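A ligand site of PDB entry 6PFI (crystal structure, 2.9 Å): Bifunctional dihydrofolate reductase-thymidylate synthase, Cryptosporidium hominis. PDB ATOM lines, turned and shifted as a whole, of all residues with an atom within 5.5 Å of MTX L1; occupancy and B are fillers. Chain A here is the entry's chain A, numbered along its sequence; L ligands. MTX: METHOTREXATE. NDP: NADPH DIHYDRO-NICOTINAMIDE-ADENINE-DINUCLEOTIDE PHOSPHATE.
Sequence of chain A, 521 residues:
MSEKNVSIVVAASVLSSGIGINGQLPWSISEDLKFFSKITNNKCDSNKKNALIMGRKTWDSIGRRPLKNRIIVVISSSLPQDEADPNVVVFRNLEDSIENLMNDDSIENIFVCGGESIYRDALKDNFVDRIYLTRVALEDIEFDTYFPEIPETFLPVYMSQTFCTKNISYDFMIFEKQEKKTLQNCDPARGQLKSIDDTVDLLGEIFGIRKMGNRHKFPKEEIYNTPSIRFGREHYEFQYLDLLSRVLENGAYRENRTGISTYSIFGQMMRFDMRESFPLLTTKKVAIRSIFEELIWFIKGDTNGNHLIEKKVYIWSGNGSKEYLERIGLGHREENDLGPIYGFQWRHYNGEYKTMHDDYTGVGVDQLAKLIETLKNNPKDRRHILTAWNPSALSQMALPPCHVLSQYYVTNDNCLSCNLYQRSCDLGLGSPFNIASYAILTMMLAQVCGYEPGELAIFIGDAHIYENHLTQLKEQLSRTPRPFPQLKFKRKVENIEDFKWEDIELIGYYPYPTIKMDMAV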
ATOM      1  N   VAL A   9      15.533  17.774  11.063  1.00  0.00           N
ATOM      2  CA  VAL A   9      16.226  16.670  10.427  1.00  0.00           C
ATOM      3  C   VAL A   9      15.399  15.416  10.656  1.00  0.00           C
ATOM      4  O   VAL A   9      15.035  15.112  11.790  1.00  0.00           O
ATOM      5  CB  VAL A   9      17.651  16.488  10.976  1.00  0.00           C
ATOM      6  CG1 VAL A   9      18.467  15.596  10.054  1.00  0.00           C
ATOM      7  CG2 VAL A   9      18.330  17.834  11.170  1.00  0.00           C
ATOM      8  N   VAL A  10      15.088  14.697   9.567  1.00  0.00           N
ATOM      9  CA  VAL A  10      14.231  13.525   9.657  1.00  0.00           C
ATOM     10  C   VAL A  10      14.540  12.600   8.484  1.00  0.00           C
ATOM     11  O   VAL A  10      14.971  13.056   7.422  1.00  0.00           O
ATOM     12  CB  VAL A  10      12.734  13.930   9.685  1.00  0.00           C
ATOM     13  CG1 VAL A  10      12.357  14.642   8.398  1.00  0.00           C
ATOM     14  CG2 VAL A  10      11.845  12.708   9.913  1.00  0.00           C
ATOM     15  N   ALA A  11      14.338  11.303   8.692  1.00  0.00           N
ATOM     16  CA  ALA A  11      14.406  10.297   7.640  1.00  0.00           C
ATOM     17  C   ALA A  11      13.088   9.550   7.625  1.00  0.00           C
ATOM     18  O   ALA A  11      12.805   8.767   8.548  1.00  0.00           O
ATOM     19  CB  ALA A  11      15.583   9.352   7.851  1.00  0.00           C
ATOM     20  N   LEU A  25      14.378   2.555  14.562  1.00  0.00           N
ATOM     21  CA  LEU A  25      14.219   2.883  13.152  1.00  0.00           C
ATOM     22  C   LEU A  25      13.760   1.652  12.364  1.00  0.00           C
ATOM     23  O   LEU A  25      14.046   0.515  12.733  1.00  0.00           O
ATOM     24  CB  LEU A  25      15.532   3.387  12.563  1.00  0.00           C
ATOM     25  CG  LEU A  25      16.186   4.612  13.209  1.00  0.00           C
ATOM     26  CD1 LEU A  25      17.486   4.937  12.498  1.00  0.00           C
ATOM     27  CD2 LEU A  25      15.248   5.806  13.189  1.00  0.00           C
ATOM     28  N   SER A  30      23.870   3.502   7.517  1.00  0.00           N
ATOM     29  CA  SER A  30      24.946   4.183   8.226  1.00  0.00           C
ATOM     30  C   SER A  30      25.254   5.546   7.620  1.00  0.00           C
ATOM     31  O   SER A  30      25.623   6.475   8.342  1.00  0.00           O
ATOM     32  CB  SER A  30      26.205   3.314   8.244  1.00  0.00           C
ATOM     33  OG  SER A  30      26.649   3.055   6.922  1.00  0.00           O
ATOM     34  N   ASP A  32      23.143   7.583   6.436  1.00  0.00           N
ATOM     35  CA  ASP A  32      22.130   8.523   6.915  1.00  0.00           C
ATOM     36  C   ASP A  32      22.491   9.080   8.284  1.00  0.00           C
ATOM     37  O   ASP A  32      22.286  10.264   8.562  1.00  0.00           O
ATOM     38  CB  ASP A  32      20.760   7.852   6.949  1.00  0.00           C
ATOM     39  CG  ASP A  32      19.685   8.727   7.554  1.00  0.00           C
ATOM     40  OD1 ASP A  32      19.590   9.923   7.164  1.00  0.00           O
ATOM     41  OD2 ASP A  32      18.933   8.228   8.417  1.00  0.00           O
ATOM     42  N   LEU A  33      23.032   8.223   9.164  1.00  0.00           N
ATOM     43  CA  LEU A  33      23.471   8.709  10.470  1.00  0.00           C
ATOM     44  C   LEU A  33      24.626   9.692  10.348  1.00  0.00           C
ATOM     45  O   LEU A  33      24.670  10.694  11.064  1.00  0.00           O
ATOM     46  CB  LEU A  33      23.863   7.531  11.362  1.00  0.00           C
ATOM     47  CG  LEU A  33      22.732   6.565  11.724  1.00  0.00           C
ATOM     48  CD1 LEU A  33      23.243   5.440  12.608  1.00  0.00           C
ATOM     49  CD2 LEU A  33      21.602   7.321  12.403  1.00  0.00           C
ATOM     50  N   LYS A  34      25.560   9.424   9.432  1.00  0.00           N
ATOM     51  CA  LYS A  34      26.646  10.376   9.195  1.00  0.00           C
ATOM     52  C   LYS A  34      26.114  11.702   8.674  1.00  0.00           C
ATOM     53  O   LYS A  34      26.645  12.760   9.012  1.00  0.00           O
ATOM     54  CB  LYS A  34      27.679   9.782   8.236  1.00  0.00           C
ATOM     55  CG  LYS A  34      28.497   8.657   8.821  1.00  0.00           C
ATOM     56  CD  LYS A  34      29.730   8.380   7.982  1.00  0.00           C
ATOM     57  CE  LYS A  34      30.635   7.361   8.659  1.00  0.00           C
ATOM     58  NZ  LYS A  34      29.966   6.040   8.857  1.00  0.00           N
ATOM     59  N   PHE A  35      25.067  11.660   7.858  1.00  0.00           N
ATOM     60  CA  PHE A  35      24.430  12.901   7.424  1.00  0.00           C
ATOM     61  C   PHE A  35      23.849  13.657   8.602  1.00  0.00           C
ATOM     62  O   PHE A  35      24.039  14.869   8.732  1.00  0.00           O
ATOM     63  CB  PHE A  35      23.355  12.620   6.372  1.00  0.00           C
ATOM     64  CG  PHE A  35      22.631  13.845   5.911  1.00  0.00           C
ATOM     65  CD1 PHE A  35      23.232  14.740   5.049  1.00  0.00           C
ATOM     66  CD2 PHE A  35      21.349  14.108   6.352  1.00  0.00           C
ATOM     67  CE1 PHE A  35      22.573  15.876   4.626  1.00  0.00           C
ATOM     68  CE2 PHE A  35      20.679  15.246   5.937  1.00  0.00           C
ATOM     69  CZ  PHE A  35      21.296  16.126   5.063  1.00  0.00           C
ATOM     70  N   PHE A  36      23.164  12.947   9.501  1.00  0.00           N
ATOM     71  CA  PHE A  36      22.664  13.581  10.718  1.00  0.00           C
ATOM     72  C   PHE A  36      23.818  14.160  11.527  1.00  0.00           C
ATOM     73  O   PHE A  36      23.695  15.225  12.141  1.00  0.00           O
ATOM     74  CB  PHE A  36      21.862  12.584  11.550  1.00  0.00           C
ATOM     75  CG  PHE A  36      21.319  13.163  12.825  1.00  0.00           C
ATOM     76  CD1 PHE A  36      20.089  13.814  12.842  1.00  0.00           C
ATOM     77  CD2 PHE A  36      22.032  13.072  14.015  1.00  0.00           C
ATOM     78  CE1 PHE A  36      19.595  14.350  14.003  1.00  0.00           C
ATOM     79  CE2 PHE A  36      21.536  13.604  15.186  1.00  0.00           C
ATOM     80  CZ  PHE A  36      20.311  14.241  15.177  1.00  0.00           C
ATOM     81  N   SER A  37      24.961  13.457  11.558  1.00  0.00           N
ATOM     82  CA  SER A  37      26.108  13.934  12.306  1.00  0.00           C
ATOM     83  C   SER A  37      26.684  15.203  11.685  1.00  0.00           C
ATOM     84  O   SER A  37      26.918  16.198  12.389  1.00  0.00           O
ATOM     85  CB  SER A  37      27.179  12.844  12.374  1.00  0.00           C
ATOM     86  OG  SER A  37      28.276  13.255  13.184  1.00  0.00           O
ATOM     87  N   THR A  40      24.276  18.412  11.832  1.00  0.00           N
ATOM     88  CA  THR A  40      24.056  19.003  13.143  1.00  0.00           C
ATOM     89  C   THR A  40      25.339  19.557  13.766  1.00  0.00           C
ATOM     90  O   THR A  40      25.256  20.337  14.720  1.00  0.00           O
ATOM     91  CB  THR A  40      23.438  17.975  14.094  1.00  0.00           C
ATOM     92  OG1 THR A  40      24.279  16.817  14.170  1.00  0.00           O
ATOM     93  CG2 THR A  40      22.055  17.564  13.609  1.00  0.00           C
ATOM     94  N   ASN A  41      26.504  19.154  13.257  1.00  0.00           N
ATOM     95  CA  ASN A  41      27.775  19.714  13.705  1.00  0.00           C
ATOM     96  C   ASN A  41      28.235  20.900  12.873  1.00  0.00           C
ATOM     97  O   ASN A  41      29.201  21.564  13.255  1.00  0.00           O
ATOM     98  CB  ASN A  41      28.861  18.625  13.679  1.00  0.00           C
ATOM     99  CG  ASN A  41      28.782  17.688  14.854  1.00  0.00           C
ATOM    100  OD1 ASN A  41      28.646  18.107  16.001  1.00  0.00           O
ATOM    101  ND2 ASN A  41      28.878  16.385  14.583  1.00  0.00           N
ATOM    102  N   MET A  54      14.834  16.862  21.067  1.00  0.00           N
ATOM    103  CA  MET A  54      14.216  15.562  20.816  1.00  0.00           C
ATOM    104  C   MET A  54      13.260  15.231  21.954  1.00  0.00           C
ATOM    105  O   MET A  54      13.335  15.787  23.048  1.00  0.00           O
ATOM    106  CB  MET A  54      15.266  14.459  20.656  1.00  0.00           C
ATOM    107  CG  MET A  54      16.184  14.284  21.853  1.00  0.00           C
ATOM    108  SD  MET A  54      17.405  12.986  21.585  1.00  0.00           S
ATOM    109  CE  MET A  54      18.236  13.588  20.124  1.00  0.00           C
ATOM    110  N   THR A  58      12.475   9.268  21.981  1.00  0.00           N
ATOM    111  CA  THR A  58      13.630   9.310  21.099  1.00  0.00           C
ATOM    112  C   THR A  58      14.933   9.361  21.902  1.00  0.00           C
ATOM    113  O   THR A  58      15.929   8.737  21.523  1.00  0.00           O
ATOM    114  CB  THR A  58      13.526  10.512  20.153  1.00  0.00           C
ATOM    115  OG1 THR A  58      12.442  10.291  19.241  1.00  0.00           O
ATOM    116  CG2 THR A  58      14.796  10.691  19.370  1.00  0.00           C
ATOM    117  N   SER A  61      15.738   5.943  22.776  1.00  0.00           N
ATOM    118  CA  SER A  61      16.122   5.098  21.661  1.00  0.00           C
ATOM    119  C   SER A  61      17.604   5.236  21.316  1.00  0.00           C
ATOM    120  O   SER A  61      18.165   4.332  20.689  1.00  0.00           O
ATOM    121  CB  SER A  61      15.263   5.402  20.438  1.00  0.00           C
ATOM    122  OG  SER A  61      15.378   6.755  20.034  1.00  0.00           O
ATOM    123  N   ILE A  62      18.235   6.334  21.692  1.00  0.00           N
ATOM    124  CA  ILE A  62      19.655   6.532  21.441  1.00  0.00           C
ATOM    125  C   ILE A  62      20.496   6.218  22.678  1.00  0.00           C
ATOM    126  O   ILE A  62      21.654   6.628  22.772  1.00  0.00           O
ATOM    127  CB  ILE A  62      19.945   7.950  20.917  1.00  0.00           C
ATOM    128  CG1 ILE A  62      19.608   9.006  21.979  1.00  0.00           C
ATOM    129  CG2 ILE A  62      19.161   8.221  19.634  1.00  0.00           C
ATOM    130  CD1 ILE A  62      20.000  10.412  21.572  1.00  0.00           C
ATOM    131  N   LEU A  67      25.702  13.315  22.606  1.00  0.00           N
ATOM    132  CA  LEU A  67      26.330  13.359  21.296  1.00  0.00           C
ATOM    133  C   LEU A  67      27.485  14.355  21.353  1.00  0.00           C
ATOM    134  O   LEU A  67      27.322  15.465  21.865  1.00  0.00           O
ATOM    135  CB  LEU A  67      25.326  13.741  20.221  1.00  0.00           C
ATOM    136  CG  LEU A  67      24.203  12.726  19.946  1.00  0.00           C
ATOM    137  CD1 LEU A  67      23.082  13.354  19.141  1.00  0.00           C
ATOM    138  CD2 LEU A  67      24.747  11.509  19.222  1.00  0.00           C
ATOM    139  N   ARG A  70      27.787  18.530  20.798  1.00  0.00           N
ATOM    140  CA  ARG A  70      26.434  19.046  20.671  1.00  0.00           C
ATOM    141  C   ARG A  70      25.710  18.953  22.006  1.00  0.00           C
ATOM    142  O   ARG A  70      25.984  18.058  22.821  1.00  0.00           O
ATOM    143  CB  ARG A  70      25.644  18.281  19.606  1.00  0.00           C
ATOM    144  CG  ARG A  70      26.087  18.564  18.178  1.00  0.00           C
ATOM    145  CD  ARG A  70      25.742  17.411  17.260  1.00  0.00           C
ATOM    146  NE  ARG A  70      26.631  16.267  17.483  1.00  0.00           N
ATOM    147  CZ  ARG A  70      26.524  15.110  16.848  1.00  0.00           C
ATOM    148  NH1 ARG A  70      25.570  14.922  15.956  1.00  0.00           N
ATOM    149  NH2 ARG A  70      27.385  14.130  17.114  1.00  0.00           N
ATOM    150  N   VAL A 112      15.598  20.199  15.251  1.00  0.00           N
ATOM    151  CA  VAL A 112      14.500  19.393  15.778  1.00  0.00           C
ATOM    152  C   VAL A 112      14.567  18.029  15.108  1.00  0.00           C
ATOM    153  O   VAL A 112      14.691  17.942  13.873  1.00  0.00           O
ATOM    154  CB  VAL A 112      13.140  20.077  15.516  1.00  0.00           C
ATOM    155  CG1 VAL A 112      11.999  19.137  15.886  1.00  0.00           C
ATOM    156  CG2 VAL A 112      13.041  21.368  16.294  1.00  0.00           C
ATOM    157  N   CYS A 113      14.482  16.971  15.910  1.00  0.00           N
ATOM    158  CA  CYS A 113      14.664  15.621  15.391  1.00  0.00           C
ATOM    159  C   CYS A 113      14.035  14.571  16.298  1.00  0.00           C
ATOM    160  O   CYS A 113      14.483  13.415  16.306  1.00  0.00           O
ATOM    161  CB  CYS A 113      16.153  15.337  15.198  1.00  0.00           C
ATOM    162  SG  CYS A 113      17.243  16.144  16.414  1.00  0.00           S
ATOM    163  N   TYR A 119       7.928  16.546  16.079  1.00  0.00           N
ATOM    164  CA  TYR A 119       7.826  17.024  14.704  1.00  0.00           C
ATOM    165  C   TYR A 119       6.498  17.728  14.467  1.00  0.00           C
ATOM    166  O   TYR A 119       6.443  18.815  13.882  1.00  0.00           O
ATOM    167  CB  TYR A 119       7.980  15.864  13.725  1.00  0.00           C
ATOM    168  CG  TYR A 119       9.399  15.384  13.508  1.00  0.00           C
ATOM    169  CD1 TYR A 119      10.457  16.276  13.450  1.00  0.00           C
ATOM    170  CD2 TYR A 119       9.669  14.035  13.371  1.00  0.00           C
ATOM    171  CE1 TYR A 119      11.748  15.835  13.263  1.00  0.00           C
ATOM    172  CE2 TYR A 119      10.952  13.578  13.175  1.00  0.00           C
ATOM    173  CZ  TYR A 119      11.991  14.476  13.126  1.00  0.00           C
ATOM    174  OH  TYR A 119      13.265  14.023  12.930  1.00  0.00           O
ATOM    175  N   TYR A 132      15.323  19.131   6.616  1.00  0.00           N
ATOM    176  CA  TYR A 132      16.244  18.199   5.965  1.00  0.00           C
ATOM    177  C   TYR A 132      15.585  16.820   5.970  1.00  0.00           C
ATOM    178  O   TYR A 132      15.525  16.165   7.024  1.00  0.00           O
ATOM    179  CB  TYR A 132      17.590  18.157   6.689  1.00  0.00           C
ATOM    180  CG  TYR A 132      18.392  19.442   6.650  1.00  0.00           C
ATOM    181  CD1 TYR A 132      19.274  19.702   5.610  1.00  0.00           C
ATOM    182  CD2 TYR A 132      18.284  20.391   7.660  1.00  0.00           C
ATOM    183  CE1 TYR A 132      20.015  20.873   5.569  1.00  0.00           C
ATOM    184  CE2 TYR A 132      19.012  21.559   7.637  1.00  0.00           C
ATOM    185  CZ  TYR A 132      19.881  21.795   6.585  1.00  0.00           C
ATOM    186  OH  TYR A 132      20.617  22.959   6.563  1.00  0.00           O
ATOM    187  N   THR A 134      15.265  12.895   4.498  1.00  0.00           N
ATOM    188  CA  THR A 134      15.941  11.760   3.868  1.00  0.00           C
ATOM    189  C   THR A 134      14.873  10.736   3.504  1.00  0.00           C
ATOM    190  O   THR A 134      14.422   9.973   4.363  1.00  0.00           O
ATOM    191  CB  THR A 134      16.982  11.163   4.819  1.00  0.00           C
ATOM    192  OG1 THR A 134      17.856  12.192   5.280  1.00  0.00           O
ATOM    193  CG2 THR A 134      17.799  10.096   4.105  1.00  0.00           C
HETATM  194  N1  MTX L   1      18.032  10.231  10.196  1.00  0.00           N
HETATM  195  C2  MTX L   1      17.766  11.487   9.788  1.00  0.00           C
HETATM  196  NA2 MTX L   1      17.974  11.823   8.401  1.00  0.00           N
HETATM  197  N3  MTX L   1      17.311  12.434  10.618  1.00  0.00           N
HETATM  198  C4  MTX L   1      17.102  12.154  11.917  1.00  0.00           C
HETATM  199  NA4 MTX L   1      16.618  13.136  12.830  1.00  0.00           N
HETATM  200  C4A MTX L   1      17.368  10.861  12.399  1.00  0.00           C
HETATM  201  N5  MTX L   1      17.173  10.544  13.709  1.00  0.00           N
HETATM  202  C6  MTX L   1      17.432   9.297  14.130  1.00  0.00           C
HETATM  203  C7  MTX L   1      17.910   8.305  13.266  1.00  0.00           C
HETATM  204  N8  MTX L   1      18.107   8.627  11.969  1.00  0.00           N
HETATM  205  C8A MTX L   1      17.843   9.905  11.515  1.00  0.00           C
HETATM  206  C9  MTX L   1      17.201   9.008  15.595  1.00  0.00           C
HETATM  207  N10 MTX L   1      18.073   9.826  16.415  1.00  0.00           N
HETATM  208  CM  MTX L   1      17.538  10.895  17.206  1.00  0.00           C
HETATM  209  C11 MTX L   1      22.242   9.122  16.257  1.00  0.00           C
HETATM  210  C12 MTX L   1      21.357   8.069  16.034  1.00  0.00           C
HETATM  211  C13 MTX L   1      19.984   8.307  16.096  1.00  0.00           C
HETATM  212  C14 MTX L   1      19.505   9.573  16.372  1.00  0.00           C
HETATM  213  C15 MTX L   1      20.394  10.633  16.576  1.00  0.00           C
HETATM  214  C16 MTX L   1      21.765  10.392  16.524  1.00  0.00           C
HETATM  215  C   MTX L   1      23.739   8.904  16.199  1.00  0.00           C
HETATM  216  O   MTX L   1      24.209   7.807  16.440  1.00  0.00           O
HETATM  217  N   MTX L   1      24.593  10.009  15.822  1.00  0.00           N
HETATM  218  CA  MTX L   1      26.014   9.879  15.713  1.00  0.00           C
HETATM  219  CT  MTX L   1      26.568  11.248  15.615  1.00  0.00           C
HETATM  220  O1  MTX L   1      25.776  12.220  15.492  1.00  0.00           O
HETATM  221  O2  MTX L   1      27.824  11.434  15.638  1.00  0.00           O
HETATM  222  CB  MTX L   1      26.303   9.187  14.436  1.00  0.00           C
HETATM  223  CG  MTX L   1      27.612   8.500  14.206  1.00  0.00           C
HETATM  224  CD  MTX L   1      27.944   8.173  12.789  1.00  0.00           C
HETATM  225  OE1 MTX L   1      28.757   8.909  12.180  1.00  0.00           O
HETATM  226  OE2 MTX L   1      27.659   7.036  12.327  1.00  0.00           O
HETATM  227  PA  NDP L   2       8.891  10.998  20.875  1.00  0.00           P
HETATM  228  O1A NDP L   2       8.216  12.077  20.056  1.00  0.00           O
HETATM  229  O2A NDP L   2      10.303  10.826  20.410  1.00  0.00           O
HETATM  230  O5B NDP L   2       8.918  11.405  22.350  1.00  0.00           O
HETATM  231  C5B NDP L   2       7.714  11.662  23.025  1.00  0.00           C
HETATM  232  C4B NDP L   2       7.820  11.959  24.467  1.00  0.00           C
HETATM  233  O4B NDP L   2       8.338  13.258  24.651  1.00  0.00           O
HETATM  234  C3B NDP L   2       6.511  11.975  25.117  1.00  0.00           C
HETATM  235  O3B NDP L   2       6.126  10.712  25.523  1.00  0.00           O
HETATM  236  C2B NDP L   2       6.758  12.832  26.241  1.00  0.00           C
HETATM  237  O2B NDP L   2       7.508  12.159  27.205  1.00  0.00           O
HETATM  238  C1B NDP L   2       7.569  13.885  25.662  1.00  0.00           C
HETATM  239  N9A NDP L   2       6.732  14.869  25.086  1.00  0.00           N
HETATM  240  C8A NDP L   2       6.302  14.888  23.793  1.00  0.00           C
HETATM  241  N7A NDP L   2       5.526  15.969  23.605  1.00  0.00           N
HETATM  242  C5A NDP L   2       5.444  16.661  24.789  1.00  0.00           C
HETATM  243  C6A NDP L   2       4.796  17.853  25.195  1.00  0.00           C
HETATM  244  N6A NDP L   2       3.985  18.604  24.213  1.00  0.00           N
HETATM  245  N1A NDP L   2       4.925  18.290  26.476  1.00  0.00           N
HETATM  246  C2A NDP L   2       5.676  17.570  27.358  1.00  0.00           C
HETATM  247  N3A NDP L   2       6.317  16.452  27.009  1.00  0.00           N
HETATM  248  C4A NDP L   2       6.218  15.967  25.718  1.00  0.00           C
HETATM  249  O3  NDP L   2       8.117   9.603  20.706  1.00  0.00           O
HETATM  250  PN  NDP L   2       7.717   9.033  19.280  1.00  0.00           P
HETATM  251  O1N NDP L   2       7.036   7.665  19.436  1.00  0.00           O
HETATM  252  O2N NDP L   2       6.733   9.968  18.608  1.00  0.00           O
HETATM  253  O5D NDP L   2       9.070   8.913  18.395  1.00  0.00           O
HETATM  254  C5D NDP L   2       9.934   7.823  18.557  1.00  0.00           C
HETATM  255  C4D NDP L   2      10.050   6.903  17.428  1.00  0.00           C
HETATM  256  O4D NDP L   2      10.338   7.657  16.256  1.00  0.00           O
HETATM  257  C3D NDP L   2      11.151   5.962  17.612  1.00  0.00           C
HETATM  258  O3D NDP L   2      10.851   4.743  17.007  1.00  0.00           O
HETATM  259  C2D NDP L   2      12.242   6.575  16.935  1.00  0.00           C
HETATM  260  O2D NDP L   2      13.161   5.631  16.487  1.00  0.00           O
HETATM  261  C1D NDP L   2      11.592   7.255  15.801  1.00  0.00           C
HETATM  262  N1N NDP L   2      12.388   8.351  15.353  1.00  0.00           N
HETATM  263  C2N NDP L   2      12.719   8.412  14.046  1.00  0.00           C
HETATM  264  C3N NDP L   2      13.504   9.464  13.547  1.00  0.00           C
HETATM  265  C7N NDP L   2      13.834   9.490  12.063  1.00  0.00           C
HETATM  266  O7N NDP L   2      14.402  10.477  11.577  1.00  0.00           O
HETATM  267  N7N NDP L   2      13.504   8.369  11.215  1.00  0.00           N
HETATM  268  C4N NDP L   2      13.956  10.475  14.416  1.00  0.00           C
HETATM  269  C5N NDP L   2      13.591  10.374  15.766  1.00  0.00           C
HETATM  270  C6N NDP L   2      12.812   9.311  16.230  1.00  0.00           C
HETATM  271  P2B NDP L   2       7.011  12.054  28.676  1.00  0.00           P
HETATM  272  O1X NDP L   2       6.357  10.672  28.855  1.00  0.00           O
HETATM  273  O2X NDP L   2       8.158  12.181  29.590  1.00  0.00           O
HETATM  274  O3X NDP L   2       6.027  13.140  28.976  1.00  0.00           O
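A nitrogen (NA2) of MTX L1 lies within hydrogen-bond range of the side-chain hydroxyl (OG1) of Thr 134.
OD1 of Asp 32 lies within hydrogen-bond range of NA2 of MTX L1 (2.8 Å).
N3 of MTX L1 is in hydrogen-bond range of N of Val 10, 3.3 Å away.
The backbone NH (N) of Thr 58 sits at hydrogen-bond distance from an oxygen (O2A) of NDP L2 (3.1 Å).
The side-chain hydroxyl (OH) of Tyr 119 sits at hydrogen-bond distance from a nitrogen (NA4) of MTX L1 (3.5 Å).
O of Val 10 lies within hydrogen-bond range of NA2 of MTX L1 (3.4 Å).
A nitrogen (N7N) of NDP L2 sits at hydrogen-bond distance from the backbone carbonyl oxygen of Ala 11 (2.8 Å).
The side-chain hydroxyl (OG) of Ser 37 lies within hydrogen-bond range of an oxygen (O2) of MTX L1 (3.1 Å).
An oxygen (O2A) of NDP L2 is in hydrogen-bond range of the side-chain hydroxyl of Thr 58 (2.5 Å).
NH1 of Arg 70 is in salt-bridge range of O1 of MTX L1 (2.7 Å).
The backbone NH (N) of Ala 11 sits at hydrogen-bond distance from an oxygen (O7N) of NDP L2 (3.0 Å).
NA4 of MTX L1 is in hydrogen-bond range of O of Val 9, at 2.7 Å.
CB of Ala 11 touches NA2 of MTX L1 (3.5 Å).
Leu 25 touches MTX L1 (CD1 to C7, 3.5 Å).
Leu 33 touches MTX L1 (CD2 to C12, 3.7 Å).
Lys 34 touches MTX L1.
Phe 36 touches MTX L1.
Thr 58 touches MTX L1.
CG2 of Ile 62 touches C14 of MTX L1, at 3.5 Å.
Leu 67 touches MTX L1 (CD2 to N, 3.7 Å).
Cys 113 touches MTX L1.
Hydrophobic or aromatic side chains within 4 Å of MTX L1: Val 9, Ala 11, Leu 25, Leu 33, Phe 36, Ile 62 and Leu 67.
16 residues have an atom within 4 Å of MTX L1: Val 9, Val 10, Ala 11, Leu 25, Asp 32, Leu 33, Lys 34, Phe 36, Ser 37, Thr 58, Ile 62, Leu 67, Arg 70, Cys 113, Tyr 119 and Thr 134.
The nearest printed residue that does not touch MTX L1 is Met 54 (4.03 Å).
N of Val 10 is in hydrogen-bond range of O of Tyr 132 (3.0 Å).
The backbone NH of Val 9 sits at hydrogen-bond distance from the backbone carbonyl oxygen of Val 112 (2.9 Å).
The side-chain carboxylate (OD1) of Asp 32 sits at hydrogen-bond distance from the side-chain hydroxyl (OG1) of Thr 134 (3.4 Å).
OG of Ser 61 sits at hydrogen-bond distance from O of Thr 58, at 2.5 Å.
OG1 of Thr 40 lies within hydrogen-bond range of O of Ser 37 (3.2 Å).
The side-chain amide nitrogen (ND2) of Asn 41 sits at hydrogen-bond distance from the backbone carbonyl oxygen (O) of Ser 37, at 2.9 Å.
OD1 of Asn 41 is in hydrogen-bond range of NE of Arg 70.
O of Phe 36 sits at hydrogen-bond distance from OG1 of Thr 40 (2.6 Å).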
